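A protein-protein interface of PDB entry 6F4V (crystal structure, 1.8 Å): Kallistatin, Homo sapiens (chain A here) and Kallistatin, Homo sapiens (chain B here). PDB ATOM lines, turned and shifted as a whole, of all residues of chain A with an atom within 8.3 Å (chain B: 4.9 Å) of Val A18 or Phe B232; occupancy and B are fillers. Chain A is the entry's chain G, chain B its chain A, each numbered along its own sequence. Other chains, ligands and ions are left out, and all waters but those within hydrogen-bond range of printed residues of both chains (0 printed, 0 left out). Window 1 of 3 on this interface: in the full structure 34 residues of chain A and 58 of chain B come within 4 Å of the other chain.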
ATOM      1  N   LEU A  10     -11.385  13.357  -5.464  1.00  0.00           N
ATOM      2  CA  LEU A  10     -10.832  12.029  -5.399  1.00  0.00           C
ATOM      3  C   LEU A  10      -9.399  12.118  -4.917  1.00  0.00           C
ATOM      4  O   LEU A  10      -8.590  12.827  -5.505  1.00  0.00           O
ATOM      5  CB  LEU A  10     -10.898  11.340  -6.768  1.00  0.00           C
ATOM      6  CG  LEU A  10     -12.282  10.834  -7.182  1.00  0.00           C
ATOM      7  CD1 LEU A  10     -12.243  10.279  -8.587  1.00  0.00           C
ATOM      8  CD2 LEU A  10     -12.844   9.787  -6.244  1.00  0.00           C
ATOM      9  N   PHE A  12      -6.294   9.617  -4.408  1.00  0.00           N
ATOM     10  CA  PHE A  12      -5.706   8.308  -4.577  1.00  0.00           C
ATOM     11  C   PHE A  12      -4.567   8.116  -3.563  1.00  0.00           C
ATOM     12  O   PHE A  12      -3.394   8.086  -3.907  1.00  0.00           O
ATOM     13  CB  PHE A  12      -5.293   8.093  -6.033  1.00  0.00           C
ATOM     14  CG  PHE A  12      -6.455   7.901  -6.955  1.00  0.00           C
ATOM     15  CD1 PHE A  12      -7.172   8.994  -7.435  1.00  0.00           C
ATOM     16  CD2 PHE A  12      -6.835   6.612  -7.372  1.00  0.00           C
ATOM     17  CE1 PHE A  12      -8.238   8.811  -8.299  1.00  0.00           C
ATOM     18  CE2 PHE A  12      -7.925   6.427  -8.213  1.00  0.00           C
ATOM     19  CZ  PHE A  12      -8.639   7.521  -8.675  1.00  0.00           C
ATOM     20  N   PRO A  15      -4.710   2.001  -1.693  1.00  0.00           N
ATOM     21  CA  PRO A  15      -4.523   1.135  -2.870  1.00  0.00           C
ATOM     22  C   PRO A  15      -5.601   1.292  -3.947  1.00  0.00           C
ATOM     23  O   PRO A  15      -6.788   1.452  -3.637  1.00  0.00           O
ATOM     24  CB  PRO A  15      -4.506  -0.252  -2.274  1.00  0.00           C
ATOM     25  CG  PRO A  15      -3.971  -0.036  -0.884  1.00  0.00           C
ATOM     26  CD  PRO A  15      -4.582   1.236  -0.439  1.00  0.00           C
ATOM     27  N   PHE A  16      -5.168   1.273  -5.207  1.00  0.00           N
ATOM     28  CA  PHE A  16      -6.065   1.450  -6.337  1.00  0.00           C
ATOM     29  C   PHE A  16      -5.648   0.595  -7.504  1.00  0.00           C
ATOM     30  O   PHE A  16      -4.511   0.104  -7.548  1.00  0.00           O
ATOM     31  CB  PHE A  16      -6.151   2.947  -6.714  1.00  0.00           C
ATOM     32  CG  PHE A  16      -4.836   3.562  -7.123  1.00  0.00           C
ATOM     33  CD1 PHE A  16      -4.004   4.173  -6.172  1.00  0.00           C
ATOM     34  CD2 PHE A  16      -4.442   3.563  -8.456  1.00  0.00           C
ATOM     35  CE1 PHE A  16      -2.812   4.767  -6.557  1.00  0.00           C
ATOM     36  CE2 PHE A  16      -3.252   4.146  -8.840  1.00  0.00           C
ATOM     37  CZ  PHE A  16      -2.434   4.751  -7.899  1.00  0.00           C
ATOM     38  N   LEU A  17      -6.568   0.431  -8.447  1.00  0.00           N
ATOM     39  CA  LEU A  17      -6.338  -0.384  -9.629  1.00  0.00           C
ATOM     40  C   LEU A  17      -6.122   0.491 -10.837  1.00  0.00           C
ATOM     41  O   LEU A  17      -6.627   1.617 -10.893  1.00  0.00           O
ATOM     42  CB  LEU A  17      -7.517  -1.294  -9.897  1.00  0.00           C
ATOM     43  CG  LEU A  17      -7.875  -2.209  -8.731  1.00  0.00           C
ATOM     44  CD1 LEU A  17      -9.255  -2.781  -8.987  1.00  0.00           C
ATOM     45  CD2 LEU A  17      -6.865  -3.333  -8.593  1.00  0.00           C
ATOM     46  N   VAL A  18      -5.400  -0.056 -11.809  1.00  0.00           N
ATOM     47  CA  VAL A  18      -5.060   0.673 -13.034  1.00  0.00           C
ATOM     48  C   VAL A  18      -5.362  -0.186 -14.241  1.00  0.00           C
ATOM     49  O   VAL A  18      -4.872  -1.288 -14.317  1.00  0.00           O
ATOM     50  CB  VAL A  18      -3.557   0.998 -13.052  1.00  0.00           C
ATOM     51  CG1 VAL A  18      -3.175   1.725 -14.331  1.00  0.00           C
ATOM     52  CG2 VAL A  18      -3.161   1.761 -11.797  1.00  0.00           C
ATOM     53  N   VAL A  19      -6.141   0.331 -15.186  1.00  0.00           N
ATOM     54  CA  VAL A  19      -6.448  -0.397 -16.432  1.00  0.00           C
ATOM     55  C   VAL A  19      -6.124   0.558 -17.585  1.00  0.00           C
ATOM     56  O   VAL A  19      -6.841   1.527 -17.773  1.00  0.00           O
ATOM     57  CB  VAL A  19      -7.922  -0.823 -16.520  1.00  0.00           C
ATOM     58  CG1 VAL A  19      -8.161  -1.733 -17.737  1.00  0.00           C
ATOM     59  CG2 VAL A  19      -8.366  -1.503 -15.238  1.00  0.00           C
ATOM     60  N   ILE A  20      -5.073   0.267 -18.336  1.00  0.00           N
ATOM     61  CA  ILE A  20      -4.706   1.091 -19.503  1.00  0.00           C
ATOM     62  C   ILE A  20      -5.299   0.390 -20.712  1.00  0.00           C
ATOM     63  O   ILE A  20      -4.984  -0.778 -20.992  1.00  0.00           O
ATOM     64  CB  ILE A  20      -3.177   1.269 -19.653  1.00  0.00           C
ATOM     65  CG1 ILE A  20      -2.608   2.007 -18.449  1.00  0.00           C
ATOM     66  CG2 ILE A  20      -2.829   2.053 -20.921  1.00  0.00           C
ATOM     67  CD1 ILE A  20      -1.105   2.018 -18.417  1.00  0.00           C
ATOM     68  N   PHE A  21      -6.128   1.139 -21.437  1.00  0.00           N
ATOM     69  CA  PHE A  21      -6.986   0.616 -22.470  1.00  0.00           C
ATOM     70  C   PHE A  21      -6.740   1.323 -23.810  1.00  0.00           C
ATOM     71  O   PHE A  21      -6.707   2.555 -23.841  1.00  0.00           O
ATOM     72  CB  PHE A  21      -8.424   0.825 -21.965  1.00  0.00           C
ATOM     73  CG  PHE A  21      -9.468   0.127 -22.765  1.00  0.00           C
ATOM     74  CD1 PHE A  21      -9.550  -1.268 -22.775  1.00  0.00           C
ATOM     75  CD2 PHE A  21     -10.416   0.870 -23.500  1.00  0.00           C
ATOM     76  CE1 PHE A  21     -10.533  -1.902 -23.518  1.00  0.00           C
ATOM     77  CE2 PHE A  21     -11.420   0.214 -24.241  1.00  0.00           C
ATOM     78  CZ  PHE A  21     -11.464  -1.162 -24.256  1.00  0.00           C
ATOM     79  N   VAL A  28      -7.004  -4.263 -23.468  1.00  0.00           N
ATOM     80  CA  VAL A  28      -6.322  -3.955 -22.227  1.00  0.00           C
ATOM     81  C   VAL A  28      -4.848  -4.128 -22.471  1.00  0.00           C
ATOM     82  O   VAL A  28      -4.348  -5.235 -22.599  1.00  0.00           O
ATOM     83  CB  VAL A  28      -6.787  -4.848 -21.051  1.00  0.00           C
ATOM     84  CG1 VAL A  28      -6.046  -4.454 -19.774  1.00  0.00           C
ATOM     85  CG2 VAL A  28      -8.298  -4.703 -20.841  1.00  0.00           C
ATOM     86  N   LEU A  29      -4.145  -3.004 -22.559  1.00  0.00           N
ATOM     87  CA  LEU A  29      -2.707  -3.010 -22.737  1.00  0.00           C
ATOM     88  C   LEU A  29      -1.948  -3.331 -21.476  1.00  0.00           C
ATOM     89  O   LEU A  29      -0.954  -4.045 -21.524  1.00  0.00           O
ATOM     90  CB  LEU A  29      -2.229  -1.688 -23.316  1.00  0.00           C
ATOM     91  CG  LEU A  29      -2.911  -1.187 -24.588  1.00  0.00           C
ATOM     92  CD1 LEU A  29      -2.360   0.178 -24.974  1.00  0.00           C
ATOM     93  CD2 LEU A  29      -2.774  -2.143 -25.759  1.00  0.00           C
ATOM     94  N   PHE A  30      -2.411  -2.808 -20.351  1.00  0.00           N
ATOM     95  CA  PHE A  30      -1.750  -3.017 -19.060  1.00  0.00           C
ATOM     96  C   PHE A  30      -2.802  -3.017 -17.974  1.00  0.00           C
ATOM     97  O   PHE A  30      -3.875  -2.375 -18.080  1.00  0.00           O
ATOM     98  CB  PHE A  30      -0.746  -1.904 -18.735  1.00  0.00           C
ATOM     99  CG  PHE A  30       0.326  -1.715 -19.750  1.00  0.00           C
ATOM    100  CD1 PHE A  30       1.497  -2.391 -19.667  1.00  0.00           C
ATOM    101  CD2 PHE A  30       0.159  -0.802 -20.772  1.00  0.00           C
ATOM    102  CE1 PHE A  30       2.484  -2.208 -20.636  1.00  0.00           C
ATOM    103  CE2 PHE A  30       1.118  -0.611 -21.740  1.00  0.00           C
ATOM    104  CZ  PHE A  30       2.300  -1.288 -21.664  1.00  0.00           C
ATOM    105  N   LEU A  31      -2.520  -3.804 -16.942  1.00  0.00           N
ATOM    106  CA  LEU A  31      -3.429  -3.950 -15.840  1.00  0.00           C
ATOM    107  C   LEU A  31      -2.632  -4.128 -14.572  1.00  0.00           C
ATOM    108  O   LEU A  31      -1.612  -4.819 -14.544  1.00  0.00           O
ATOM    109  CB  LEU A  31      -4.300  -5.194 -16.128  1.00  0.00           C
ATOM    110  CG  LEU A  31      -5.342  -5.655 -15.179  1.00  0.00           C
ATOM    111  CD1 LEU A  31      -6.332  -4.549 -14.808  1.00  0.00           C
ATOM    112  CD2 LEU A  31      -6.074  -6.839 -15.853  1.00  0.00           C
ATOM    113  N   GLY A  32      -3.087  -3.505 -13.507  1.00  0.00           N
ATOM    114  CA  GLY A  32      -2.384  -3.641 -12.286  1.00  0.00           C
ATOM    115  C   GLY A  32      -3.041  -2.995 -11.097  1.00  0.00           C
ATOM    116  O   GLY A  32      -4.169  -2.521 -11.158  1.00  0.00           O
ATOM    117  N   LYS A  33      -2.307  -3.083 -10.001  1.00  0.00           N
ATOM    118  CA  LYS A  33      -2.715  -2.593  -8.717  1.00  0.00           C
ATOM    119  C   LYS A  33      -1.528  -1.951  -8.015  1.00  0.00           C
ATOM    120  O   LYS A  33      -0.455  -2.564  -7.901  1.00  0.00           O
ATOM    121  CB  LYS A  33      -3.212  -3.729  -7.843  1.00  0.00           C
ATOM    122  CG  LYS A  33      -3.623  -3.289  -6.441  1.00  0.00           C
ATOM    123  CD  LYS A  33      -4.340  -4.379  -5.648  1.00  0.00           C
ATOM    124  CE  LYS A  33      -3.541  -5.654  -5.566  1.00  0.00           C
ATOM    125  NZ  LYS A  33      -4.256  -6.665  -4.751  1.00  0.00           N
ATOM    126  N   VAL A  34      -1.776  -0.781  -7.463  1.00  0.00           N
ATOM    127  CA  VAL A  34      -0.817  -0.065  -6.617  1.00  0.00           C
ATOM    128  C   VAL A  34      -1.256  -0.268  -5.163  1.00  0.00           C
ATOM    129  O   VAL A  34      -2.283   0.237  -4.738  1.00  0.00           O
ATOM    130  CB  VAL A  34      -0.775   1.445  -6.939  1.00  0.00           C
ATOM    131  CG1 VAL A  34       0.248   2.163  -6.045  1.00  0.00           C
ATOM    132  CG2 VAL A  34      -0.466   1.700  -8.409  1.00  0.00           C
ATOM    133  N   PHE B  30       1.568  -5.563 -11.761  1.00  0.00           N
ATOM    134  CA  PHE B  30       1.575  -4.856 -13.036  1.00  0.00           C
ATOM    135  C   PHE B  30       2.011  -5.758 -14.153  1.00  0.00           C
ATOM    136  O   PHE B  30       3.083  -6.322 -14.106  1.00  0.00           O
ATOM    137  CB  PHE B  30       2.435  -3.556 -13.011  1.00  0.00           C
ATOM    138  CG  PHE B  30       2.128  -2.647 -14.158  1.00  0.00           C
ATOM    139  CD1 PHE B  30       0.882  -1.994 -14.233  1.00  0.00           C
ATOM    140  CD2 PHE B  30       3.026  -2.489 -15.196  1.00  0.00           C
ATOM    141  CE1 PHE B  30       0.579  -1.184 -15.322  1.00  0.00           C
ATOM    142  CE2 PHE B  30       2.698  -1.704 -16.300  1.00  0.00           C
ATOM    143  CZ  PHE B  30       1.481  -1.049 -16.348  1.00  0.00           C
ATOM    144  N   TRP B 173      -1.098  12.972 -20.940  1.00  0.00           N
ATOM    145  CA  TRP B 173      -2.460  13.228 -20.459  1.00  0.00           C
ATOM    146  C   TRP B 173      -3.152  14.253 -21.350  1.00  0.00           C
ATOM    147  O   TRP B 173      -2.524  15.243 -21.719  1.00  0.00           O
ATOM    148  CB  TRP B 173      -2.446  13.833 -19.053  1.00  0.00           C
ATOM    149  CG  TRP B 173      -1.824  13.034 -17.997  1.00  0.00           C
ATOM    150  CD1 TRP B 173      -0.807  13.402 -17.202  1.00  0.00           C
ATOM    151  CD2 TRP B 173      -2.215  11.722 -17.580  1.00  0.00           C
ATOM    152  NE1 TRP B 173      -0.530  12.415 -16.292  1.00  0.00           N
ATOM    153  CE2 TRP B 173      -1.367  11.357 -16.520  1.00  0.00           C
ATOM    154  CE3 TRP B 173      -3.218  10.826 -17.990  1.00  0.00           C
ATOM    155  CZ2 TRP B 173      -1.483  10.112 -15.861  1.00  0.00           C
ATOM    156  CZ3 TRP B 173      -3.326   9.592 -17.329  1.00  0.00           C
ATOM    157  CH2 TRP B 173      -2.461   9.255 -16.295  1.00  0.00           C
ATOM    158  N   SER B 218     -14.916   4.264  -6.290  1.00  0.00           N
ATOM    159  CA  SER B 218     -15.043   5.276  -7.316  1.00  0.00           C
ATOM    160  C   SER B 218     -14.178   4.908  -8.517  1.00  0.00           C
ATOM    161  O   SER B 218     -13.222   4.166  -8.393  1.00  0.00           O
ATOM    162  CB  SER B 218     -14.625   6.638  -6.760  1.00  0.00           C
ATOM    163  OG  SER B 218     -15.448   7.030  -5.666  1.00  0.00           O
ATOM    164  N   VAL B 219     -14.512   5.445  -9.675  1.00  0.00           N
ATOM    165  CA  VAL B 219     -13.800   5.157 -10.911  1.00  0.00           C
ATOM    166  C   VAL B 219     -13.566   6.475 -11.638  1.00  0.00           C
ATOM    167  O   VAL B 219     -14.493   7.260 -11.825  1.00  0.00           O
ATOM    168  CB  VAL B 219     -14.620   4.194 -11.805  1.00  0.00           C
ATOM    169  CG1 VAL B 219     -13.893   3.869 -13.112  1.00  0.00           C
ATOM    170  CG2 VAL B 219     -14.960   2.905 -11.045  1.00  0.00           C
ATOM    171  N   LEU B 220     -12.316   6.706 -12.014  1.00  0.00           N
ATOM    172  CA  LEU B 220     -11.877   7.858 -12.804  1.00  0.00           C
ATOM    173  C   LEU B 220     -11.395   7.326 -14.119  1.00  0.00           C
ATOM    174  O   LEU B 220     -10.609   6.370 -14.133  1.00  0.00           O
ATOM    175  CB  LEU B 220     -10.703   8.541 -12.083  1.00  0.00           C
ATOM    176  CG  LEU B 220      -9.925   9.619 -12.865  1.00  0.00           C
ATOM    177  CD1 LEU B 220     -10.819  10.798 -13.241  1.00  0.00           C
ATOM    178  CD2 LEU B 220      -8.772  10.115 -12.019  1.00  0.00           C
ATOM    179  N   MET B 222      -9.154   8.730 -17.228  1.00  0.00           N
ATOM    180  CA  MET B 222      -8.363   9.823 -17.777  1.00  0.00           C
ATOM    181  C   MET B 222      -7.954   9.494 -19.201  1.00  0.00           C
ATOM    182  O   MET B 222      -7.494   8.381 -19.512  1.00  0.00           O
ATOM    183  CB  MET B 222      -7.130  10.109 -16.925  1.00  0.00           C
ATOM    184  CG  MET B 222      -7.466  10.729 -15.597  1.00  0.00           C
ATOM    185  SD  MET B 222      -5.999  11.062 -14.606  1.00  0.00           S
ATOM    186  CE  MET B 222      -5.352  12.471 -15.494  1.00  0.00           C
ATOM    187  N   VAL B 230      -7.049   5.493 -19.466  1.00  0.00           N
ATOM    188  CA  VAL B 230      -6.745   4.720 -18.263  1.00  0.00           C
ATOM    189  C   VAL B 230      -7.899   4.868 -17.292  1.00  0.00           C
ATOM    190  O   VAL B 230      -8.384   5.975 -17.053  1.00  0.00           O
ATOM    191  CB  VAL B 230      -5.382   5.124 -17.623  1.00  0.00           C
ATOM    192  CG1 VAL B 230      -5.316   6.594 -17.238  1.00  0.00           C
ATOM    193  CG2 VAL B 230      -5.047   4.264 -16.403  1.00  0.00           C
ATOM    194  N   PHE B 231      -8.296   3.740 -16.692  1.00  0.00           N
ATOM    195  CA  PHE B 231      -9.183   3.725 -15.563  1.00  0.00           C
ATOM    196  C   PHE B 231      -8.372   3.547 -14.286  1.00  0.00           C
ATOM    197  O   PHE B 231      -7.601   2.572 -14.151  1.00  0.00           O
ATOM    198  CB  PHE B 231     -10.189   2.580 -15.686  1.00  0.00           C
ATOM    199  CG  PHE B 231     -11.047   2.652 -16.906  1.00  0.00           C
ATOM    200  CD1 PHE B 231     -10.567   2.238 -18.127  1.00  0.00           C
ATOM    201  CD2 PHE B 231     -12.342   3.144 -16.821  1.00  0.00           C
ATOM    202  CE1 PHE B 231     -11.347   2.305 -19.263  1.00  0.00           C
ATOM    203  CE2 PHE B 231     -13.152   3.194 -17.956  1.00  0.00           C
ATOM    204  CZ  PHE B 231     -12.640   2.803 -19.177  1.00  0.00           C
ATOM    205  N   PHE B 232      -8.567   4.484 -13.352  1.00  0.00           N
ATOM    206  CA  PHE B 232      -8.081   4.388 -12.016  1.00  0.00           C
ATOM    207  C   PHE B 232      -9.300   4.093 -11.127  1.00  0.00           C
ATOM    208  O   PHE B 232     -10.216   4.916 -11.014  1.00  0.00           O
ATOM    209  CB  PHE B 232      -7.392   5.685 -11.569  1.00  0.00           C
ATOM    210  CG  PHE B 232      -6.083   5.987 -12.276  1.00  0.00           C
ATOM    211  CD1 PHE B 232      -4.970   5.190 -12.095  1.00  0.00           C
ATOM    212  CD2 PHE B 232      -5.963   7.082 -13.118  1.00  0.00           C
ATOM    213  CE1 PHE B 232      -3.758   5.500 -12.706  1.00  0.00           C
ATOM    214  CE2 PHE B 232      -4.768   7.386 -13.737  1.00  0.00           C
ATOM    215  CZ  PHE B 232      -3.674   6.587 -13.547  1.00  0.00           C
ATOM    216  N   ILE B 233      -9.292   2.911 -10.518  1.00  0.00           N
ATOM    217  CA  ILE B 233     -10.390   2.410  -9.722  1.00  0.00           C
ATOM    218  C   ILE B 233      -9.946   2.430  -8.284  1.00  0.00           C
ATOM    219  O   ILE B 233      -8.927   1.851  -7.919  1.00  0.00           O
ATOM    220  CB  ILE B 233     -10.808   1.009 -10.155  1.00  0.00           C
ATOM    221  CG1 ILE B 233     -11.249   1.058 -11.618  1.00  0.00           C
ATOM    222  CG2 ILE B 233     -11.940   0.499  -9.282  1.00  0.00           C
ATOM    223  CD1 ILE B 233     -10.738  -0.098 -12.431  1.00  0.00           C
ATOM    224  N   LEU B 234     -10.715   3.162  -7.486  1.00  0.00           N
ATOM    225  CA  LEU B 234     -10.362   3.456  -6.105  1.00  0.00           C
ATOM    226  C   LEU B 234     -11.347   2.782  -5.152  1.00  0.00           C
ATOM    227  O   LEU B 234     -12.405   3.347  -4.887  1.00  0.00           O
ATOM    228  CB  LEU B 234     -10.394   4.964  -5.910  1.00  0.00           C
ATOM    229  CG  LEU B 234      -9.927   5.474  -4.544  1.00  0.00           C
ATOM    230  CD1 LEU B 234      -8.496   5.055  -4.252  1.00  0.00           C
ATOM    231  CD2 LEU B 234     -10.062   6.981  -4.490  1.00  0.00           C
ATOM    232  N   LEU B 272      -3.396  12.542  -7.155  1.00  0.00           N
ATOM    233  CA  LEU B 272      -2.967  11.293  -7.769  1.00  0.00           C
ATOM    234  C   LEU B 272      -1.479  11.187  -7.584  1.00  0.00           C
ATOM    235  O   LEU B 272      -0.775  12.153  -7.872  1.00  0.00           O
ATOM    236  CB  LEU B 272      -3.340  11.268  -9.239  1.00  0.00           C
ATOM    237  CG  LEU B 272      -3.015   9.994 -10.056  1.00  0.00           C
ATOM    238  CD1 LEU B 272      -3.882   8.819  -9.614  1.00  0.00           C
ATOM    239  CD2 LEU B 272      -3.201  10.269 -11.549  1.00  0.00           C
ATOM    240  N   LEU B 322       5.389   0.488 -14.813  1.00  0.00           N
ATOM    241  CA  LEU B 322       4.462   1.628 -14.913  1.00  0.00           C
ATOM    242  C   LEU B 322       5.109   2.844 -14.269  1.00  0.00           C
ATOM    243  O   LEU B 322       5.587   2.740 -13.132  1.00  0.00           O
ATOM    244  CB  LEU B 322       3.180   1.333 -14.120  1.00  0.00           C
ATOM    245  CG  LEU B 322       2.086   2.426 -14.093  1.00  0.00           C
ATOM    246  CD1 LEU B 322       1.647   2.774 -15.501  1.00  0.00           C
ATOM    247  CD2 LEU B 322       0.897   1.992 -13.259  1.00  0.00           C
ATOM    248  N   VAL B 324       4.002   6.919 -13.747  1.00  0.00           N
ATOM    249  CA  VAL B 324       2.983   7.939 -13.820  1.00  0.00           C
ATOM    250  C   VAL B 324       3.565   9.235 -13.268  1.00  0.00           C
ATOM    251  O   VAL B 324       4.094   9.277 -12.144  1.00  0.00           O
ATOM    252  CB  VAL B 324       1.725   7.501 -13.023  1.00  0.00           C
ATOM    253  CG1 VAL B 324       0.768   8.660 -12.786  1.00  0.00           C
ATOM    254  CG2 VAL B 324       1.032   6.328 -13.762  1.00  0.00           C
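Phe A12 touches Phe B232 (CE2 to CB, 3.5 Å). Phe A12 touches Leu B234 (CE2 to CB, 3.7 Å). CG of Phe A12 touches CD1 of Leu B272, 3.8 Å away. Phe A16 touches Phe B232. Leu A17 touches Phe B231 (O to O, 3.5 Å). Val A18 touches Val B230 (CG1 to CG2, 3.8 Å). Phe B231 touches Val A18. Ile B233 touches Val A19. CZ of Phe B30 touches CB of Phe A30, 3.4 Å away. Leu A31 touches Phe B30.
N of Phe B231 sits at hydrogen-bond distance from O of Val A19. O of Ile B233 is in hydrogen-bond range of N of Leu A17 (2.8 Å).
Printed residues of chain B within 4 Å of Phe A12: Leu B220, Phe B232, Leu B234 and Leu B272. Of chain B, only Val B230, Phe B231 and Phe B232 come within 4 Å of Val A18. Phe B232 touches just these residues of chain A: Phe A12, Phe A16, Leu A17 and Val A18. Of the printed residues of chain A, Leu B234 touches Phe A12 (3.7 Å). The nearest residue of chain A that does not touch Phe B232 is Val A19 (5.1 Å).
O of Ser B218 sits at hydrogen-bond distance from N of Leu B234 (2.8 Å). N of Met B222 is in hydrogen-bond range of O of Val B230 (2.9 Å). The backbone NH (N) of Val A34 sits at hydrogen-bond distance from the backbone carbonyl oxygen (O) of Phe A16, at 2.9 Å. The backbone NH (N) of Val A18 is in hydrogen-bond range of the backbone carbonyl oxygen (O) of Gly A32 (2.8 Å). N of Leu A29 is in hydrogen-bond range of O of Ile A20. The backbone carbonyl oxygen (O) of Phe A30 sits at hydrogen-bond distance from the backbone NH (N) of Ile A20.
Printed residues of chain A that touch a printed residue of chain B: Leu A10, Phe A12, Phe A16, Leu A17, Val A18, Val A19, Ile A20, Phe A30 and Leu A31. Hydrophobic or aromatic side chains of chain A within 4 Å of the printed part of chain B: Leu A10, Phe A12, Phe A16, Leu A17, Val A18, Val A19, Ile A20 and Phe A30. Of the 14 printed residues of chain B, 9 touch a printed residue of chain A. Hydrophobic or aromatic side chains of chain B within 4 Å of the printed part of chain A: Phe B30, Leu B220, Val B230, Phe B231, Phe B232, Ile B233, Leu B234 and Leu B272. Among the printed residues, no Asp or Glu carboxylate lies within 4 Å of a Lys or Arg side-chain nitrogen of the other chain.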
